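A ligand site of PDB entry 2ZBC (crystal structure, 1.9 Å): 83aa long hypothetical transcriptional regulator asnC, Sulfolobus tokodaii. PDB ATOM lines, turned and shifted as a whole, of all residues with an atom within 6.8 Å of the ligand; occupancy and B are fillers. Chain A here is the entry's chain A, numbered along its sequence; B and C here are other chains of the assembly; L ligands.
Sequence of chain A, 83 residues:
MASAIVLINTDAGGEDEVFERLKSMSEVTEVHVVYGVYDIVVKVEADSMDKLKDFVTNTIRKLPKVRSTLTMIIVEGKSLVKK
Residues that only touch the ligand: Glu 15, Val 56 of chain B, Tyr 35, Lys 53 of chain B, Thr 57 of chain B, Arg 61 of chain B and Leu 70 of chain B. Hydrophobic or aromatic side chains within 4 Å of the ligand: Tyr 35 and Val 56 of chain B. Within 4 Å of the ligand: Glu 15, Val 34, Tyr 35, Gly 36, Tyr 38, Asp 39, Lys 53 of chain B, Val 56 of chain B, Thr 57 of chain B, Arg 61 of chain B, Thr 69 of chain B, Leu 70 of chain B and Thr 71 of chain B. The nearest printed residue that does not touch the ligand is Val 33 (4.3 Å).
The backbone carbonyl oxygen (O) of Val 34 is in hydrogen-bond range of a nitrogen (N1) of the ligand (3.0 Å). The backbone NH of Thr 71 of chain B lies within hydrogen-bond range of an oxygen (O1) of the ligand (2.9 Å). N of Gly 36 lies within hydrogen-bond range of O1 of the ligand. An oxygen (O2) of the ligand sits at hydrogen-bond distance from the side-chain hydroxyl (OG1) of Thr 69 of chain B (2.6 Å). OD1 of Asp 39 lies within salt-bridge range of N1 of the ligand (2.8 Å). A nitrogen (N1) of the ligand sits at hydrogen-bond distance from the backbone carbonyl oxygen (O) of Tyr 38 (2.9 Å). OG1 of Thr 71 of chain B lies within hydrogen-bond range of O2 of the ligand (3.0 Å). A nitrogen (N1) of the ligand lies within hydrogen-bond range of the backbone carbonyl oxygen (O) of Gly 36, at 2.9 Å.
The side-chain amino group of Lys 53 of chain B is in hydrogen-bond range of the side-chain hydroxyl of Thr 57 of chain B (2.8 Å). NH2 of Arg 61 of chain B lies within salt-bridge range of OD2 of Asp 39 (3.2 Å). The guanidinium group (NH1) of Arg 61 of chain B sits at hydrogen-bond distance from the side-chain hydroxyl (OG1) of Thr 69 of chain B, at 2.7 Å. The side-chain carboxylate of Glu 15 is in salt-bridge range of the guanidinium group of Arg 61 of chain B (2.9 Å). The guanidinium group of Arg 61 of chain B lies within hydrogen-bond range of the side-chain hydroxyl of Thr 10 (3.4 Å). The backbone carbonyl oxygen of Asp 39 is in hydrogen-bond range of the backbone NH of Val 34 (3.0 Å). N of Glu 15 sits at hydrogen-bond distance from OG1 of Thr 10, at 3.4 Å. O of Leu 70 of chain B sits at hydrogen-bond distance from N of Leu 7 of chain B (2.7 Å).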
ATOM      1  N   ASN A   9      37.199  -7.034  13.991  1.00  0.00           N
ATOM      2  CA  ASN A   9      36.551  -8.338  13.957  1.00  0.00           C
ATOM      3  C   ASN A   9      37.599  -9.307  14.341  1.00  0.00           C
ATOM      4  O   ASN A   9      38.731  -9.247  13.819  1.00  0.00           O
ATOM      5  CB  ASN A   9      35.956  -8.734  12.584  1.00  0.00           C
ATOM      6  CG  ASN A   9      34.586  -8.075  12.341  1.00  0.00           C
ATOM      7  OD1 ASN A   9      33.468  -8.678  12.549  1.00  0.00           O
ATOM      8  ND2 ASN A   9      34.647  -6.852  11.864  1.00  0.00           N
ATOM      9  N   THR A  10      37.207 -10.260  15.190  1.00  0.00           N
ATOM     10  CA  THR A  10      38.145 -11.314  15.630  1.00  0.00           C
ATOM     11  C   THR A  10      37.772 -12.647  14.981  1.00  0.00           C
ATOM     12  O   THR A  10      36.709 -12.768  14.398  1.00  0.00           O
ATOM     13  CB  THR A  10      38.097 -11.506  17.146  1.00  0.00           C
ATOM     14  OG1 THR A  10      36.810 -11.951  17.587  1.00  0.00           O
ATOM     15  CG2 THR A  10      38.318 -10.194  17.871  1.00  0.00           C
ATOM     16  N   GLU A  15      37.196 -12.851  20.819  1.00  0.00           N
ATOM     17  CA  GLU A  15      36.941 -11.473  21.252  1.00  0.00           C
ATOM     18  C   GLU A  15      37.394 -11.105  22.694  1.00  0.00           C
ATOM     19  O   GLU A  15      37.909 -10.016  22.889  1.00  0.00           O
ATOM     20  CB  GLU A  15      35.518 -10.996  20.976  1.00  0.00           C
ATOM     21  CG  GLU A  15      34.396 -11.789  21.611  1.00  0.00           C
ATOM     22  CD  GLU A  15      33.968 -12.953  20.758  1.00  0.00           C
ATOM     23  OE1 GLU A  15      32.888 -13.429  20.950  1.00  0.00           O
ATOM     24  OE2 GLU A  15      34.712 -13.379  19.907  1.00  0.00           O
ATOM     25  N   ASP A  16      37.183 -11.980  23.678  1.00  0.00           N
ATOM     26  CA  ASP A  16      37.594 -11.666  25.062  1.00  0.00           C
ATOM     27  C   ASP A  16      39.100 -11.589  25.221  1.00  0.00           C
ATOM     28  O   ASP A  16      39.631 -10.743  25.984  1.00  0.00           O
ATOM     29  CB  ASP A  16      36.995 -12.669  26.063  1.00  0.00           C
ATOM     30  CG  ASP A  16      35.466 -12.645  26.099  1.00  0.00           C
ATOM     31  OD1 ASP A  16      34.821 -11.775  25.476  1.00  0.00           O
ATOM     32  OD2 ASP A  16      34.831 -13.489  26.744  1.00  0.00           O
ATOM     33  N   VAL A  33      33.762  -4.630  23.932  1.00  0.00           N
ATOM     34  CA  VAL A  33      33.194  -5.662  23.016  1.00  0.00           C
ATOM     35  C   VAL A  33      31.735  -5.257  22.800  1.00  0.00           C
ATOM     36  O   VAL A  33      31.037  -4.771  23.720  1.00  0.00           O
ATOM     37  CB  VAL A  33      33.253  -7.097  23.632  1.00  0.00           C
ATOM     38  CG1 VAL A  33      32.705  -8.244  22.783  1.00  0.00           C
ATOM     39  CG2 VAL A  33      34.647  -7.463  24.007  1.00  0.00           C
ATOM     40  N   VAL A  34      31.245  -5.576  21.610  1.00  0.00           N
ATOM     41  CA  VAL A  34      29.966  -5.158  21.096  1.00  0.00           C
ATOM     42  C   VAL A  34      29.250  -6.220  20.309  1.00  0.00           C
ATOM     43  O   VAL A  34      29.849  -7.074  19.685  1.00  0.00           O
ATOM     44  CB  VAL A  34      30.064  -3.902  20.211  1.00  0.00           C
ATOM     45  CG1 VAL A  34      30.340  -2.628  21.016  1.00  0.00           C
ATOM     46  CG2 VAL A  34      31.015  -4.110  19.065  1.00  0.00           C
ATOM     47  N   TYR A  35      27.906  -6.187  20.417  1.00  0.00           N
ATOM     48  CA  TYR A  35      26.983  -6.967  19.538  1.00  0.00           C
ATOM     49  C   TYR A  35      26.822  -6.281  18.196  1.00  0.00           C
ATOM     50  O   TYR A  35      26.778  -5.031  18.064  1.00  0.00           O
ATOM     51  CB  TYR A  35      25.621  -7.147  20.182  1.00  0.00           C
ATOM     52  CG  TYR A  35      25.651  -7.880  21.489  1.00  0.00           C
ATOM     53  CD1 TYR A  35      25.690  -9.254  21.533  1.00  0.00           C
ATOM     54  CD2 TYR A  35      25.600  -7.193  22.700  1.00  0.00           C
ATOM     55  CE1 TYR A  35      25.744  -9.919  22.703  1.00  0.00           C
ATOM     56  CE2 TYR A  35      25.594  -7.892  23.892  1.00  0.00           C
ATOM     57  CZ  TYR A  35      25.666  -9.238  23.883  1.00  0.00           C
ATOM     58  OH  TYR A  35      25.680  -9.923  25.061  1.00  0.00           O
ATOM     59  N   GLY A  36      26.962  -7.081  17.181  1.00  0.00           N
ATOM     60  CA  GLY A  36      26.589  -6.774  15.823  1.00  0.00           C
ATOM     61  C   GLY A  36      27.732  -7.105  14.896  1.00  0.00           C
ATOM     62  O   GLY A  36      28.557  -8.002  15.123  1.00  0.00           O
ATOM     63  N   VAL A  37      27.730  -6.393  13.775  1.00  0.00           N
ATOM     64  CA  VAL A  37      28.639  -6.786  12.695  1.00  0.00           C
ATOM     65  C   VAL A  37      30.162  -6.671  12.987  1.00  0.00           C
ATOM     66  O   VAL A  37      30.970  -7.323  12.352  1.00  0.00           O
ATOM     67  CB  VAL A  37      28.174  -6.160  11.389  1.00  0.00           C
ATOM     68  CG1 VAL A  37      28.514  -4.762  11.282  1.00  0.00           C
ATOM     69  CG2 VAL A  37      28.707  -6.997  10.197  1.00  0.00           C
ATOM     70  N   TYR A  38      30.524  -5.877  13.967  1.00  0.00           N
ATOM     71  CA  TYR A  38      31.875  -5.795  14.506  1.00  0.00           C
ATOM     72  C   TYR A  38      31.878  -6.319  15.958  1.00  0.00           C
ATOM     73  O   TYR A  38      30.810  -6.454  16.594  1.00  0.00           O
ATOM     74  CB  TYR A  38      32.374  -4.288  14.464  1.00  0.00           C
ATOM     75  CG  TYR A  38      32.143  -3.658  13.151  1.00  0.00           C
ATOM     76  CD1 TYR A  38      32.978  -3.909  12.081  1.00  0.00           C
ATOM     77  CD2 TYR A  38      31.071  -2.800  12.946  1.00  0.00           C
ATOM     78  CE1 TYR A  38      32.748  -3.340  10.894  1.00  0.00           C
ATOM     79  CE2 TYR A  38      30.835  -2.224  11.756  1.00  0.00           C
ATOM     80  CZ  TYR A  38      31.664  -2.511  10.726  1.00  0.00           C
ATOM     81  OH  TYR A  38      31.327  -1.953   9.503  1.00  0.00           O
ATOM     82  N   ASP A  39      33.060  -6.670  16.432  1.00  0.00           N
ATOM     83  CA  ASP A  39      33.232  -7.367  17.650  1.00  0.00           C
ATOM     84  C   ASP A  39      33.844  -6.524  18.734  1.00  0.00           C
ATOM     85  O   ASP A  39      33.445  -6.701  19.915  1.00  0.00           O
ATOM     86  CB  ASP A  39      34.150  -8.501  17.461  1.00  0.00           C
ATOM     87  CG  ASP A  39      33.577  -9.523  16.449  1.00  0.00           C
ATOM     88  OD1 ASP A  39      32.343  -9.599  16.347  1.00  0.00           O
ATOM     89  OD2 ASP A  39      34.343 -10.186  15.715  1.00  0.00           O
ATOM     90  N   ILE A  40      34.776  -5.651  18.366  1.00  0.00           N
ATOM     91  CA  ILE A  40      35.363  -4.720  19.350  1.00  0.00           C
ATOM     92  C   ILE A  40      35.548  -3.333  18.759  1.00  0.00           C
ATOM     93  O   ILE A  40      35.849  -3.183  17.556  1.00  0.00           O
ATOM     94  CB  ILE A  40      36.762  -5.221  19.722  1.00  0.00           C
ATOM     95  CG1 ILE A  40      36.732  -6.619  20.363  1.00  0.00           C
ATOM     96  CG2 ILE A  40      37.517  -4.239  20.583  1.00  0.00           C
ATOM     97  CD1 ILE A  40      38.087  -7.202  20.678  1.00  0.00           C
ATOM     98  N   VAL B   6      20.529 -14.234  15.921  1.00  0.00           N
ATOM     99  CA  VAL B   6      21.939 -14.272  15.477  1.00  0.00           C
ATOM    100  C   VAL B   6      22.028 -14.742  14.074  1.00  0.00           C
ATOM    101  O   VAL B   6      21.451 -15.799  13.754  1.00  0.00           O
ATOM    102  CB  VAL B   6      22.772 -15.175  16.360  1.00  0.00           C
ATOM    103  CG1 VAL B   6      24.255 -15.063  16.070  1.00  0.00           C
ATOM    104  CG2 VAL B   6      22.510 -14.901  17.775  1.00  0.00           C
ATOM    105  N   LEU B   7      22.672 -13.915  13.242  1.00  0.00           N
ATOM    106  CA  LEU B   7      22.964 -14.225  11.846  1.00  0.00           C
ATOM    107  C   LEU B   7      24.369 -14.881  11.733  1.00  0.00           C
ATOM    108  O   LEU B   7      25.370 -14.329  12.127  1.00  0.00           O
ATOM    109  CB  LEU B   7      22.813 -13.015  10.972  1.00  0.00           C
ATOM    110  CG  LEU B   7      21.459 -12.347  11.113  1.00  0.00           C
ATOM    111  CD1 LEU B   7      21.382 -11.090  10.265  1.00  0.00           C
ATOM    112  CD2 LEU B   7      20.328 -13.365  10.760  1.00  0.00           C
ATOM    113  N   LEU B  52      23.607 -14.503  27.734  1.00  0.00           N
ATOM    114  CA  LEU B  52      23.608 -14.396  26.263  1.00  0.00           C
ATOM    115  C   LEU B  52      25.025 -14.234  25.721  1.00  0.00           C
ATOM    116  O   LEU B  52      25.449 -14.870  24.761  1.00  0.00           O
ATOM    117  CB  LEU B  52      22.667 -13.278  25.813  1.00  0.00           C
ATOM    118  CG  LEU B  52      22.809 -12.988  24.288  1.00  0.00           C
ATOM    119  CD1 LEU B  52      22.036 -13.994  23.547  1.00  0.00           C
ATOM    120  CD2 LEU B  52      22.299 -11.662  23.974  1.00  0.00           C
ATOM    121  N   LYS B  53      25.817 -13.338  26.350  1.00  0.00           N
ATOM    122  CA  LYS B  53      27.165 -13.085  25.914  1.00  0.00           C
ATOM    123  C   LYS B  53      28.001 -14.332  25.989  1.00  0.00           C
ATOM    124  O   LYS B  53      28.776 -14.638  25.120  1.00  0.00           O
ATOM    125  CB  LYS B  53      27.826 -11.998  26.820  1.00  0.00           C
ATOM    126  CG  LYS B  53      29.299 -11.941  26.715  1.00  0.00           C
ATOM    127  CD  LYS B  53      29.733 -11.511  25.330  1.00  0.00           C
ATOM    128  CE  LYS B  53      31.172 -11.123  25.285  1.00  0.00           C
ATOM    129  NZ  LYS B  53      32.132 -12.269  25.467  1.00  0.00           N
ATOM    130  N   VAL B  56      26.899 -16.778  23.159  1.00  0.00           N
ATOM    131  CA  VAL B  56      27.375 -16.359  21.851  1.00  0.00           C
ATOM    132  C   VAL B  56      28.856 -16.577  21.721  1.00  0.00           C
ATOM    133  O   VAL B  56      29.316 -17.228  20.741  1.00  0.00           O
ATOM    134  CB  VAL B  56      26.958 -14.858  21.561  1.00  0.00           C
ATOM    135  CG1 VAL B  56      27.671 -14.316  20.313  1.00  0.00           C
ATOM    136  CG2 VAL B  56      25.458 -14.719  21.515  1.00  0.00           C
ATOM    137  N   THR B  57      29.630 -16.081  22.713  1.00  0.00           N
ATOM    138  CA  THR B  57      31.105 -16.116  22.617  1.00  0.00           C
ATOM    139  C   THR B  57      31.719 -17.470  22.839  1.00  0.00           C
ATOM    140  O   THR B  57      32.595 -17.879  22.063  1.00  0.00           O
ATOM    141  CB  THR B  57      31.766 -15.151  23.583  1.00  0.00           C
ATOM    142  OG1 THR B  57      31.567 -13.797  23.140  1.00  0.00           O
ATOM    143  CG2 THR B  57      33.292 -15.386  23.541  1.00  0.00           C
ATOM    144  N   ARG B  61      30.244 -19.135  18.915  1.00  0.00           N
ATOM    145  CA  ARG B  61      31.370 -18.706  18.147  1.00  0.00           C
ATOM    146  C   ARG B  61      32.610 -19.609  18.332  1.00  0.00           C
ATOM    147  O   ARG B  61      33.663 -19.306  17.800  1.00  0.00           O
ATOM    148  CB  ARG B  61      31.728 -17.230  18.510  1.00  0.00           C
ATOM    149  CG  ARG B  61      30.701 -16.286  18.017  1.00  0.00           C
ATOM    150  CD  ARG B  61      30.793 -14.904  18.617  1.00  0.00           C
ATOM    151  NE  ARG B  61      32.087 -14.209  18.311  1.00  0.00           N
ATOM    152  CZ  ARG B  61      32.398 -13.588  17.228  1.00  0.00           C
ATOM    153  NH1 ARG B  61      31.571 -13.573  16.210  1.00  0.00           N
ATOM    154  NH2 ARG B  61      33.613 -12.947  17.136  1.00  0.00           N
ATOM    155  N   SER B  68      31.535 -16.440  11.224  1.00  0.00           N
ATOM    156  CA  SER B  68      31.146 -15.186  11.853  1.00  0.00           C
ATOM    157  C   SER B  68      29.737 -15.227  12.358  1.00  0.00           C
ATOM    158  O   SER B  68      28.907 -16.094  11.960  1.00  0.00           O
ATOM    159  CB  SER B  68      31.388 -14.044  10.886  1.00  0.00           C
ATOM    160  OG  SER B  68      30.568 -14.119   9.815  1.00  0.00           O
ATOM    161  N   THR B  69      29.503 -14.339  13.303  1.00  0.00           N
ATOM    162  CA  THR B  69      28.162 -14.099  13.848  1.00  0.00           C
ATOM    163  C   THR B  69      27.841 -12.619  13.967  1.00  0.00           C
ATOM    164  O   THR B  69      28.725 -11.778  14.246  1.00  0.00           O
ATOM    165  CB  THR B  69      27.974 -14.716  15.192  1.00  0.00           C
ATOM    166  OG1 THR B  69      28.882 -14.128  16.125  1.00  0.00           O
ATOM    167  CG2 THR B  69      28.296 -16.187  15.252  1.00  0.00           C
ATOM    168  N   LEU B  70      26.564 -12.345  13.776  1.00  0.00           N
ATOM    169  CA  LEU B  70      25.984 -11.024  13.923  1.00  0.00           C
ATOM    170  C   LEU B  70      24.779 -11.136  14.799  1.00  0.00           C
ATOM    171  O   LEU B  70      23.731 -11.644  14.370  1.00  0.00           O
ATOM    172  CB  LEU B  70      25.607 -10.475  12.549  1.00  0.00           C
ATOM    173  CG  LEU B  70      25.325  -8.979  12.346  1.00  0.00           C
ATOM    174  CD1 LEU B  70      25.258  -8.568  10.902  1.00  0.00           C
ATOM    175  CD2 LEU B  70      24.133  -8.551  13.134  1.00  0.00           C
ATOM    176  N   THR B  71      24.899 -10.722  16.059  1.00  0.00           N
ATOM    177  CA  THR B  71      23.843 -10.783  17.027  1.00  0.00           C
ATOM    178  C   THR B  71      23.082  -9.496  16.998  1.00  0.00           C
ATOM    179  O   THR B  71      23.684  -8.444  17.221  1.00  0.00           O
ATOM    180  CB  THR B  71      24.460 -10.982  18.425  1.00  0.00           C
ATOM    181  OG1 THR B  71      25.165 -12.247  18.467  1.00  0.00           O
ATOM    182  CG2 THR B  71      23.413 -11.067  19.479  1.00  0.00           C
ATOM    183  N   MET B  72      21.779  -9.610  16.789  1.00  0.00           N
ATOM    184  CA  MET B  72      20.813  -8.528  16.846  1.00  0.00           C
ATOM    185  C   MET B  72      20.011  -8.652  18.148  1.00  0.00           C
ATOM    186  O   MET B  72      19.141  -9.577  18.325  1.00  0.00           O
ATOM    187  CB  MET B  72      19.932  -8.583  15.598  1.00  0.00           C
ATOM    188  CG  MET B  72      20.695  -8.636  14.331  1.00  0.00           C
ATOM    189  SD  MET B  72      19.435  -8.649  12.791  1.00  0.00           S
ATOM    190  CE  MET B  72      18.856 -10.615  12.838  1.00  0.00           C
ATOM    191  N   VAL C  75      28.935  -4.707  25.600  1.00  0.00           N
ATOM    192  CA  VAL C  75      28.788  -5.841  26.483  1.00  0.00           C
ATOM    193  C   VAL C  75      29.204  -5.430  27.903  1.00  0.00           C
ATOM    194  O   VAL C  75      30.332  -5.072  28.123  1.00  0.00           O
ATOM    195  CB  VAL C  75      29.740  -7.041  26.093  1.00  0.00           C
ATOM    196  CG1 VAL C  75      29.710  -8.099  27.215  1.00  0.00           C
ATOM    197  CG2 VAL C  75      29.350  -7.661  24.781  1.00  0.00           C
HETATM  198  N1  LIG L   1      29.868  -9.096  17.443  1.00  0.00           N
HETATM  199  C1  LIG L   1      29.590 -10.537  17.749  1.00  0.00           C
HETATM  200  C2  LIG L   1      28.176 -10.897  17.561  1.00  0.00           C
HETATM  201  O1  LIG L   1      27.367  -9.946  17.424  1.00  0.00           O
HETATM  202  C3  LIG L   1      30.106 -10.954  19.140  1.00  0.00           C
HETATM  203  C4  LIG L   1      29.235 -10.422  20.298  1.00  0.00           C
HETATM  204  C5  LIG L   1      31.519 -10.592  19.285  1.00  0.00           C
HETATM  205  C6  LIG L   1      29.635 -10.992  21.668  1.00  0.00           C
HETATM  206  O2  LIG L   1      27.959 -12.109  17.492  1.00  0.00           O
